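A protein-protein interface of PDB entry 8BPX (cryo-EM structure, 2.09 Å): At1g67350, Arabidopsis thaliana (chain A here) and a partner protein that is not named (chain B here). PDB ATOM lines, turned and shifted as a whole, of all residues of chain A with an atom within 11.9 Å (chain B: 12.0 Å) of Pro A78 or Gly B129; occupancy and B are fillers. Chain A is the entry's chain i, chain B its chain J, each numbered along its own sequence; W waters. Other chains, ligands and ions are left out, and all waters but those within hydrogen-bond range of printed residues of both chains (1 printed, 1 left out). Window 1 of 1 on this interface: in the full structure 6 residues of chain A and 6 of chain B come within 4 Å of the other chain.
Trp B134 touches Ala A73. CH2 of Trp B134 touches N of Gly A74 (3.9 Å). Pro A78 touches Ala B128 (CB to CB, 3.8 Å). CB of Pro A78 touches N of Gly B129, at 3.8 Å. CG1 of Val B126 touches OH of Tyr A79 (3.9 Å). Tyr A79 touches Ala B128 (CE1 to CB, 3.8 Å). Leu A82 touches Ala B128.
Water W1 lies within hydrogen-bond range of N of Ala B128, OH of Tyr A79 and N of Tyr B127.
Of the 15 printed residues of chain A, 5 touch a printed residue of chain B. Printed residues of chain A that touch a printed residue of chain B: Ala A73, Gly A74, Pro A78, Tyr A79 and Leu A82. Hydrophobic or aromatic side chains of chain A within 4 Å of the printed part of chain B: Pro A78, Tyr A79 and Leu A82. Of the 15 printed residues of chain B, 4 touch a printed residue of chain A. Hydrophobic or aromatic side chains of chain B within 4 Å of the printed part of chain A: Val B126, Ala B128 and Trp B134. Among the printed residues, 7 pairs touch across the chains.
Ser A70 touches none of the printed residues of chain B. Of the printed residues of chain B, Ala A73 touches Trp B134 (3.8 Å). Printed residues of chain B within 4 Å of Gly A74: Trp B134 (3.9 Å). No residue of chain B comes within 4 Å of Asp A77. Tyr A79 touches just these residues of chain B: Val B126 and Ala B128. No residue of chain B comes within 4 Å of Asp A80. No residue of chain B comes within 4 Å of Asp A81. Leu A82 touches just one residue of chain B: Ala B128. Val B126 touches just one residue of chain A: Tyr A79 (3.9 Å). Ala B128 touches three residues of chain A. Gly B129 touches just one residue of chain A: Pro A78. No residue of chain A comes within 4 Å of Lys B130. No residue of chain A comes within 4 Å of Ser B133. Of the printed residues of chain A, Trp B134 touches Ala A73 (3.8 Å) and Gly A74 (3.9 Å). Thr B135 touches none of the printed residues of chain A. The nearest residue of chain A that does not touch Gly B129 is Leu A82 (6.0 Å). The nearest printed residue of chain A that does not touch Trp B134 is Arg A75 (6.3 Å).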
ATOM      1  N   SER A  70     -10.464  -1.521  10.652  1.00  0.00           N
ATOM      2  CA  SER A  70     -11.507  -0.585  10.250  1.00  0.00           C
ATOM      3  C   SER A  70     -12.206  -0.994   8.959  1.00  0.00           C
ATOM      4  O   SER A  70     -13.300  -0.495   8.681  1.00  0.00           O
ATOM      5  CB  SER A  70     -10.917   0.822  10.106  1.00  0.00           C
ATOM      6  OG  SER A  70     -10.047   0.897   8.994  1.00  0.00           O
ATOM      7  N   GLN A  71     -11.609  -1.882   8.170  1.00  0.00           N
ATOM      8  CA  GLN A  71     -12.202  -2.358   6.929  1.00  0.00           C
ATOM      9  C   GLN A  71     -12.842  -3.734   7.077  1.00  0.00           C
ATOM     10  O   GLN A  71     -13.191  -4.355   6.071  1.00  0.00           O
ATOM     11  CB  GLN A  71     -11.147  -2.387   5.821  1.00  0.00           C
ATOM     12  CG  GLN A  71     -11.019  -1.091   5.035  1.00  0.00           C
ATOM     13  CD  GLN A  71     -11.367   0.132   5.859  1.00  0.00           C
ATOM     14  OE1 GLN A  71     -10.625   0.524   6.756  1.00  0.00           O
ATOM     15  NE2 GLN A  71     -12.509   0.737   5.561  1.00  0.00           N
ATOM     16  N   VAL A  72     -13.001  -4.219   8.303  1.00  0.00           N
ATOM     17  CA  VAL A  72     -13.512  -5.564   8.542  1.00  0.00           C
ATOM     18  C   VAL A  72     -15.033  -5.546   8.484  1.00  0.00           C
ATOM     19  O   VAL A  72     -15.681  -4.681   9.086  1.00  0.00           O
ATOM     20  CB  VAL A  72     -13.009  -6.100   9.892  1.00  0.00           C
ATOM     21  CG1 VAL A  72     -13.781  -7.344  10.299  1.00  0.00           C
ATOM     22  CG2 VAL A  72     -11.514  -6.380   9.826  1.00  0.00           C
ATOM     23  N   ALA A  73     -15.606  -6.505   7.758  1.00  0.00           N
ATOM     24  CA  ALA A  73     -17.056  -6.617   7.672  1.00  0.00           C
ATOM     25  C   ALA A  73     -17.656  -6.812   9.059  1.00  0.00           C
ATOM     26  O   ALA A  73     -17.217  -7.673   9.825  1.00  0.00           O
ATOM     27  CB  ALA A  73     -17.444  -7.773   6.752  1.00  0.00           C
ATOM     28  N   GLY A  74     -18.662  -6.004   9.374  1.00  0.00           N
ATOM     29  CA  GLY A  74     -19.262  -5.958  10.688  1.00  0.00           C
ATOM     30  C   GLY A  74     -19.060  -4.646  11.416  1.00  0.00           C
ATOM     31  O   GLY A  74     -19.784  -4.373  12.379  1.00  0.00           O
ATOM     32  N   ARG A  75     -18.102  -3.818  10.981  1.00  0.00           N
ATOM     33  CA  ARG A  75     -17.875  -2.533  11.632  1.00  0.00           C
ATOM     34  C   ARG A  75     -17.590  -1.415  10.632  1.00  0.00           C
ATOM     35  O   ARG A  75     -17.085  -0.359  11.027  1.00  0.00           O
ATOM     36  CB  ARG A  75     -16.728  -2.633  12.649  1.00  0.00           C
ATOM     37  CG  ARG A  75     -15.385  -3.006  12.051  1.00  0.00           C
ATOM     38  CD  ARG A  75     -14.393  -3.408  13.129  1.00  0.00           C
ATOM     39  NE  ARG A  75     -13.956  -2.275  13.935  1.00  0.00           N
ATOM     40  CZ  ARG A  75     -14.329  -2.058  15.188  1.00  0.00           C
ATOM     41  NH1 ARG A  75     -15.157  -2.879  15.815  1.00  0.00           N
ATOM     42  NH2 ARG A  75     -13.862  -0.991  15.827  1.00  0.00           N
ATOM     43  N   ARG A  76     -17.910  -1.611   9.360  1.00  0.00           N
ATOM     44  CA  ARG A  76     -17.671  -0.608   8.334  1.00  0.00           C
ATOM     45  C   ARG A  76     -18.837   0.366   8.233  1.00  0.00           C
ATOM     46  O   ARG A  76     -19.991   0.016   8.495  1.00  0.00           O
ATOM     47  CB  ARG A  76     -17.445  -1.277   6.980  1.00  0.00           C
ATOM     48  CG  ARG A  76     -16.447  -2.408   7.031  1.00  0.00           C
ATOM     49  CD  ARG A  76     -16.051  -2.854   5.651  1.00  0.00           C
ATOM     50  NE  ARG A  76     -15.301  -1.824   4.945  1.00  0.00           N
ATOM     51  CZ  ARG A  76     -15.114  -1.809   3.632  1.00  0.00           C
ATOM     52  NH1 ARG A  76     -15.600  -2.761   2.856  1.00  0.00           N
ATOM     53  NH2 ARG A  76     -14.424  -0.812   3.089  1.00  0.00           N
ATOM     54  N   ASP A  77     -18.519   1.600   7.858  1.00  0.00           N
ATOM     55  CA  ASP A  77     -19.551   2.540   7.452  1.00  0.00           C
ATOM     56  C   ASP A  77     -20.270   1.969   6.233  1.00  0.00           C
ATOM     57  O   ASP A  77     -19.610   1.481   5.308  1.00  0.00           O
ATOM     58  CB  ASP A  77     -18.930   3.905   7.132  1.00  0.00           C
ATOM     59  CG  ASP A  77     -19.967   4.978   6.791  1.00  0.00           C
ATOM     60  OD1 ASP A  77     -21.181   4.697   6.812  1.00  0.00           O
ATOM     61  OD2 ASP A  77     -19.566   6.123   6.514  1.00  0.00           O
ATOM     62  N   PRO A  78     -21.606   1.992   6.199  1.00  0.00           N
ATOM     63  CA  PRO A  78     -22.317   1.380   5.064  1.00  0.00           C
ATOM     64  C   PRO A  78     -21.945   1.964   3.712  1.00  0.00           C
ATOM     65  O   PRO A  78     -22.022   1.251   2.704  1.00  0.00           O
ATOM     66  CB  PRO A  78     -23.797   1.626   5.402  1.00  0.00           C
ATOM     67  CG  PRO A  78     -23.801   2.633   6.510  1.00  0.00           C
ATOM     68  CD  PRO A  78     -22.532   2.416   7.260  1.00  0.00           C
ATOM     69  N   TYR A  79     -21.524   3.229   3.653  1.00  0.00           N
ATOM     70  CA  TYR A  79     -21.178   3.830   2.372  1.00  0.00           C
ATOM     71  C   TYR A  79     -19.843   3.333   1.818  1.00  0.00           C
ATOM     72  O   TYR A  79     -19.580   3.520   0.627  1.00  0.00           O
ATOM     73  CB  TYR A  79     -21.166   5.352   2.498  1.00  0.00           C
ATOM     74  CG  TYR A  79     -22.557   5.935   2.553  1.00  0.00           C
ATOM     75  CD1 TYR A  79     -23.404   5.847   1.456  1.00  0.00           C
ATOM     76  CD2 TYR A  79     -23.033   6.547   3.704  1.00  0.00           C
ATOM     77  CE1 TYR A  79     -24.680   6.364   1.499  1.00  0.00           C
ATOM     78  CE2 TYR A  79     -24.309   7.065   3.755  1.00  0.00           C
ATOM     79  CZ  TYR A  79     -25.127   6.972   2.650  1.00  0.00           C
ATOM     80  OH  TYR A  79     -26.399   7.487   2.690  1.00  0.00           O
ATOM     81  N   ASP A  80     -19.000   2.710   2.646  1.00  0.00           N
ATOM     82  CA  ASP A  80     -17.734   2.174   2.150  1.00  0.00           C
ATOM     83  C   ASP A  80     -17.946   1.063   1.132  1.00  0.00           C
ATOM     84  O   ASP A  80     -17.160   0.928   0.188  1.00  0.00           O
ATOM     85  CB  ASP A  80     -16.882   1.664   3.311  1.00  0.00           C
ATOM     86  CG  ASP A  80     -16.885   2.604   4.488  1.00  0.00           C
ATOM     87  OD1 ASP A  80     -17.225   3.785   4.291  1.00  0.00           O
ATOM     88  OD2 ASP A  80     -16.559   2.166   5.610  1.00  0.00           O
ATOM     89  N   ASP A  81     -18.989   0.252   1.306  1.00  0.00           N
ATOM     90  CA  ASP A  81     -19.252  -0.819   0.355  1.00  0.00           C
ATOM     91  C   ASP A  81     -19.750  -0.266  -0.977  1.00  0.00           C
ATOM     92  O   ASP A  81     -19.426  -0.809  -2.038  1.00  0.00           O
ATOM     93  CB  ASP A  81     -20.256  -1.806   0.944  1.00  0.00           C
ATOM     94  CG  ASP A  81     -19.829  -3.248   0.762  1.00  0.00           C
ATOM     95  OD1 ASP A  81     -18.901  -3.497  -0.037  1.00  0.00           O
ATOM     96  OD2 ASP A  81     -20.421  -4.133   1.415  1.00  0.00           O
ATOM     97  N   LEU A  82     -20.539   0.811  -0.942  1.00  0.00           N
ATOM     98  CA  LEU A  82     -21.055   1.402  -2.172  1.00  0.00           C
ATOM     99  C   LEU A  82     -19.957   2.006  -3.036  1.00  0.00           C
ATOM    100  O   LEU A  82     -20.099   2.039  -4.262  1.00  0.00           O
ATOM    101  CB  LEU A  82     -22.092   2.483  -1.858  1.00  0.00           C
ATOM    102  CG  LEU A  82     -23.507   2.055  -1.466  1.00  0.00           C
ATOM    103  CD1 LEU A  82     -23.969   0.911  -2.340  1.00  0.00           C
ATOM    104  CD2 LEU A  82     -23.600   1.679  -0.005  1.00  0.00           C
ATOM    105  N   LEU A  83     -18.876   2.488  -2.430  1.00  0.00           N
ATOM    106  CA  LEU A  83     -17.811   3.145  -3.173  1.00  0.00           C
ATOM    107  C   LEU A  83     -16.602   2.254  -3.408  1.00  0.00           C
ATOM    108  O   LEU A  83     -15.710   2.643  -4.168  1.00  0.00           O
ATOM    109  CB  LEU A  83     -17.379   4.420  -2.444  1.00  0.00           C
ATOM    110  CG  LEU A  83     -18.341   5.584  -2.679  1.00  0.00           C
ATOM    111  CD1 LEU A  83     -17.833   6.865  -2.044  1.00  0.00           C
ATOM    112  CD2 LEU A  83     -18.568   5.778  -4.166  1.00  0.00           C
ATOM    113  N   GLU A  84     -16.553   1.077  -2.794  1.00  0.00           N
ATOM    114  CA  GLU A  84     -15.436   0.160  -2.997  1.00  0.00           C
ATOM    115  C   GLU A  84     -15.885  -1.083  -3.758  1.00  0.00           C
ATOM    116  O   GLU A  84     -15.110  -1.676  -4.510  1.00  0.00           O
ATOM    117  CB  GLU A  84     -14.816  -0.238  -1.656  1.00  0.00           C
ATOM    118  CG  GLU A  84     -13.760   0.730  -1.145  1.00  0.00           C
ATOM    119  CD  GLU A  84     -12.449   0.618  -1.899  1.00  0.00           C
ATOM    120  OE1 GLU A  84     -12.093  -0.508  -2.311  1.00  0.00           O
ATOM    121  OE2 GLU A  84     -11.774   1.653  -2.077  1.00  0.00           O
ATOM    122  N   TYR B 124     -35.687   9.061   9.629  1.00  0.00           N
ATOM    123  CA  TYR B 124     -34.814   9.136   8.465  1.00  0.00           C
ATOM    124  C   TYR B 124     -34.354   7.735   8.080  1.00  0.00           C
ATOM    125  O   TYR B 124     -33.872   6.981   8.929  1.00  0.00           O
ATOM    126  CB  TYR B 124     -33.609  10.032   8.758  1.00  0.00           C
ATOM    127  CG  TYR B 124     -32.676  10.225   7.584  1.00  0.00           C
ATOM    128  CD1 TYR B 124     -33.161  10.627   6.345  1.00  0.00           C
ATOM    129  CD2 TYR B 124     -31.312  10.003   7.713  1.00  0.00           C
ATOM    130  CE1 TYR B 124     -32.316  10.803   5.274  1.00  0.00           C
ATOM    131  CE2 TYR B 124     -30.459  10.175   6.644  1.00  0.00           C
ATOM    132  CZ  TYR B 124     -30.966  10.574   5.426  1.00  0.00           C
ATOM    133  OH  TYR B 124     -30.120  10.745   4.363  1.00  0.00           O
ATOM    134  N   THR B 125     -34.500   7.394   6.803  1.00  0.00           N
ATOM    135  CA  THR B 125     -34.152   6.072   6.293  1.00  0.00           C
ATOM    136  C   THR B 125     -32.850   6.153   5.508  1.00  0.00           C
ATOM    137  O   THR B 125     -32.734   6.947   4.570  1.00  0.00           O
ATOM    138  CB  THR B 125     -35.268   5.514   5.410  1.00  0.00           C
ATOM    139  OG1 THR B 125     -36.415   5.227   6.218  1.00  0.00           O
ATOM    140  CG2 THR B 125     -34.815   4.249   4.707  1.00  0.00           C
ATOM    141  N   VAL B 126     -31.880   5.329   5.891  1.00  0.00           N
ATOM    142  CA  VAL B 126     -30.625   5.176   5.164  1.00  0.00           C
ATOM    143  C   VAL B 126     -30.677   3.827   4.464  1.00  0.00           C
ATOM    144  O   VAL B 126     -30.598   2.777   5.115  1.00  0.00           O
ATOM    145  CB  VAL B 126     -29.408   5.272   6.095  1.00  0.00           C
ATOM    146  CG1 VAL B 126     -28.115   5.200   5.290  1.00  0.00           C
ATOM    147  CG2 VAL B 126     -29.470   6.541   6.922  1.00  0.00           C
ATOM    148  N   TYR B 127     -30.810   3.844   3.137  1.00  0.00           N
ATOM    149  CA  TYR B 127     -30.923   2.592   2.402  1.00  0.00           C
ATOM    150  C   TYR B 127     -29.587   1.867   2.278  1.00  0.00           C
ATOM    151  O   TYR B 127     -29.576   0.679   1.944  1.00  0.00           O
ATOM    152  CB  TYR B 127     -31.504   2.838   1.007  1.00  0.00           C
ATOM    153  CG  TYR B 127     -32.925   3.352   0.968  1.00  0.00           C
ATOM    154  CD1 TYR B 127     -33.998   2.482   1.067  1.00  0.00           C
ATOM    155  CD2 TYR B 127     -33.192   4.705   0.792  1.00  0.00           C
ATOM    156  CE1 TYR B 127     -35.297   2.943   1.022  1.00  0.00           C
ATOM    157  CE2 TYR B 127     -34.488   5.177   0.743  1.00  0.00           C
ATOM    158  CZ  TYR B 127     -35.540   4.288   0.857  1.00  0.00           C
ATOM    159  OH  TYR B 127     -36.837   4.737   0.811  1.00  0.00           O
ATOM    160  N   ALA B 128     -28.470   2.549   2.547  1.00  0.00           N
ATOM    161  CA  ALA B 128     -27.160   1.935   2.351  1.00  0.00           C
ATOM    162  C   ALA B 128     -26.981   0.708   3.237  1.00  0.00           C
ATOM    163  O   ALA B 128     -26.453  -0.319   2.793  1.00  0.00           O
ATOM    164  CB  ALA B 128     -26.055   2.955   2.616  1.00  0.00           C
ATOM    165  N   GLY B 129     -27.423   0.788   4.490  1.00  0.00           N
ATOM    166  CA  GLY B 129     -27.335  -0.354   5.381  1.00  0.00           C
ATOM    167  C   GLY B 129     -28.329  -1.460   5.093  1.00  0.00           C
ATOM    168  O   GLY B 129     -28.258  -2.510   5.739  1.00  0.00           O
ATOM    169  N   LYS B 130     -29.238  -1.257   4.141  1.00  0.00           N
ATOM    170  CA  LYS B 130     -30.285  -2.222   3.828  1.00  0.00           C
ATOM    171  C   LYS B 130     -29.998  -3.053   2.583  1.00  0.00           C
ATOM    172  O   LYS B 130     -30.812  -3.911   2.231  1.00  0.00           O
ATOM    173  CB  LYS B 130     -31.629  -1.505   3.657  1.00  0.00           C
ATOM    174  CG  LYS B 130     -32.319  -1.130   4.951  1.00  0.00           C
ATOM    175  CD  LYS B 130     -33.451  -0.151   4.705  1.00  0.00           C
ATOM    176  CE  LYS B 130     -33.838   0.579   5.975  1.00  0.00           C
ATOM    177  NZ  LYS B 130     -35.139   0.101   6.504  1.00  0.00           N
ATOM    178  N   VAL B 131     -28.877  -2.809   1.899  1.00  0.00           N
ATOM    179  CA  VAL B 131     -28.558  -3.571   0.694  1.00  0.00           C
ATOM    180  C   VAL B 131     -28.293  -5.030   1.045  1.00  0.00           C
ATOM    181  O   VAL B 131     -28.780  -5.945   0.377  1.00  0.00           O
ATOM    182  CB  VAL B 131     -27.357  -2.934  -0.034  1.00  0.00           C
ATOM    183  CG1 VAL B 131     -26.786  -3.883  -1.077  1.00  0.00           C
ATOM    184  CG2 VAL B 131     -27.742  -1.592  -0.655  1.00  0.00           C
ATOM    185  N   ARG B 132     -27.526  -5.264   2.106  1.00  0.00           N
ATOM    186  CA  ARG B 132     -27.169  -6.599   2.599  1.00  0.00           C
ATOM    187  C   ARG B 132     -27.333  -6.603   4.112  1.00  0.00           C
ATOM    188  O   ARG B 132     -26.378  -6.327   4.842  1.00  0.00           O
ATOM    189  CB  ARG B 132     -25.750  -6.978   2.201  1.00  0.00           C
ATOM    190  CG  ARG B 132     -25.318  -8.362   2.658  1.00  0.00           C
ATOM    191  CD  ARG B 132     -23.945  -8.712   2.181  1.00  0.00           C
ATOM    192  NE  ARG B 132     -23.505 -10.043   2.580  1.00  0.00           N
ATOM    193  CZ  ARG B 132     -22.416 -10.636   2.117  1.00  0.00           C
ATOM    194  NH1 ARG B 132     -21.636 -10.044   1.227  1.00  0.00           N
ATOM    195  NH2 ARG B 132     -22.094 -11.845   2.570  1.00  0.00           N
ATOM    196  N   SER B 133     -28.530  -6.947   4.574  1.00  0.00           N
ATOM    197  CA  SER B 133     -28.796  -6.978   6.002  1.00  0.00           C
ATOM    198  C   SER B 133     -28.277  -8.274   6.611  1.00  0.00           C
ATOM    199  O   SER B 133     -28.319  -9.334   5.982  1.00  0.00           O
ATOM    200  CB  SER B 133     -30.294  -6.827   6.274  1.00  0.00           C
ATOM    201  OG  SER B 133     -31.052  -7.646   5.399  1.00  0.00           O
ATOM    202  N   TRP B 134     -27.770  -8.174   7.833  1.00  0.00           N
ATOM    203  CA  TRP B 134     -27.254  -9.317   8.571  1.00  0.00           C
ATOM    204  C   TRP B 134     -28.292  -9.799   9.573  1.00  0.00           C
ATOM    205  O   TRP B 134     -28.923  -8.994  10.261  1.00  0.00           O
ATOM    206  CB  TRP B 134     -25.964  -8.958   9.313  1.00  0.00           C
ATOM    207  CG  TRP B 134     -24.726  -9.020   8.478  1.00  0.00           C
ATOM    208  CD1 TRP B 134     -24.648  -8.986   7.114  1.00  0.00           C
ATOM    209  CD2 TRP B 134     -23.377  -9.128   8.953  1.00  0.00           C
ATOM    210  NE1 TRP B 134     -23.336  -9.067   6.712  1.00  0.00           N
ATOM    211  CE2 TRP B 134     -22.536  -9.155   7.822  1.00  0.00           C
ATOM    212  CE3 TRP B 134     -22.801  -9.209  10.224  1.00  0.00           C
ATOM    213  CZ2 TRP B 134     -21.149  -9.254   7.926  1.00  0.00           C
ATOM    214  CZ3 TRP B 134     -21.425  -9.308  10.325  1.00  0.00           C
ATOM    215  CH2 TRP B 134     -20.615  -9.327   9.184  1.00  0.00           C
ATOM    216  N   THR B 135     -28.457 -11.115   9.660  1.00  0.00           N
ATOM    217  CA  THR B 135     -29.257 -11.673  10.738  1.00  0.00           C
ATOM    218  C   THR B 135     -28.526 -11.527  12.073  1.00  0.00           C
ATOM    219  O   THR B 135     -27.308 -11.342  12.129  1.00  0.00           O
ATOM    220  CB  THR B 135     -29.580 -13.147  10.471  1.00  0.00           C
ATOM    221  OG1 THR B 135     -28.401 -13.941  10.645  1.00  0.00           O
ATOM    222  CG2 THR B 135     -30.114 -13.334   9.055  1.00  0.00           C
ATOM    223  N   ASN B 136     -29.302 -11.588  13.157  1.00  0.00           N
ATOM    224  CA  ASN B 136     -28.724 -11.662  14.497  1.00  0.00           C
ATOM    225  C   ASN B 136     -27.709 -12.797  14.582  1.00  0.00           C
ATOM    226  O   ASN B 136     -26.614 -12.633  15.142  1.00  0.00           O
ATOM    227  CB  ASN B 136     -29.858 -11.845  15.515  1.00  0.00           C
ATOM    228  CG  ASN B 136     -29.371 -11.913  16.953  1.00  0.00           C
ATOM    229  OD1 ASN B 136     -30.022 -12.522  17.801  1.00  0.00           O
ATOM    230  ND2 ASN B 136     -28.241 -11.280  17.239  1.00  0.00           N
ATOM    231  N   GLU B 138     -25.801 -14.273  12.176  1.00  0.00           N
ATOM    232  CA  GLU B 138     -24.520 -14.070  11.511  1.00  0.00           C
ATOM    233  C   GLU B 138     -23.734 -12.904  12.104  1.00  0.00           C
ATOM    234  O   GLU B 138     -22.500 -12.948  12.112  1.00  0.00           O
ATOM    235  CB  GLU B 138     -24.722 -13.917  10.002  1.00  0.00           C
ATOM    236  CG  GLU B 138     -25.567 -12.765   9.535  1.00  0.00           C
ATOM    237  CD  GLU B 138     -26.374 -13.132   8.293  1.00  0.00           C
ATOM    238  OE1 GLU B 138     -26.234 -14.271   7.807  1.00  0.00           O
ATOM    239  OE2 GLU B 138     -27.147 -12.290   7.803  1.00  0.00           O
ATOM    240  N   THR B 139     -24.411 -11.893  12.654  1.00  0.00           N
ATOM    241  CA  THR B 139     -23.690 -10.847  13.377  1.00  0.00           C
ATOM    242  C   THR B 139     -22.979 -11.411  14.601  1.00  0.00           C
ATOM    243  O   THR B 139     -21.829 -11.051  14.877  1.00  0.00           O
ATOM    244  CB  THR B 139     -24.640  -9.713  13.774  1.00  0.00           C
ATOM    245  OG1 THR B 139     -25.444  -9.333  12.651  1.00  0.00           O
ATOM    246  CG2 THR B 139     -23.851  -8.500  14.262  1.00  0.00           C
HETATM  247  O   HOH W   1     -28.271   5.307   1.931  1.00  0.00           O
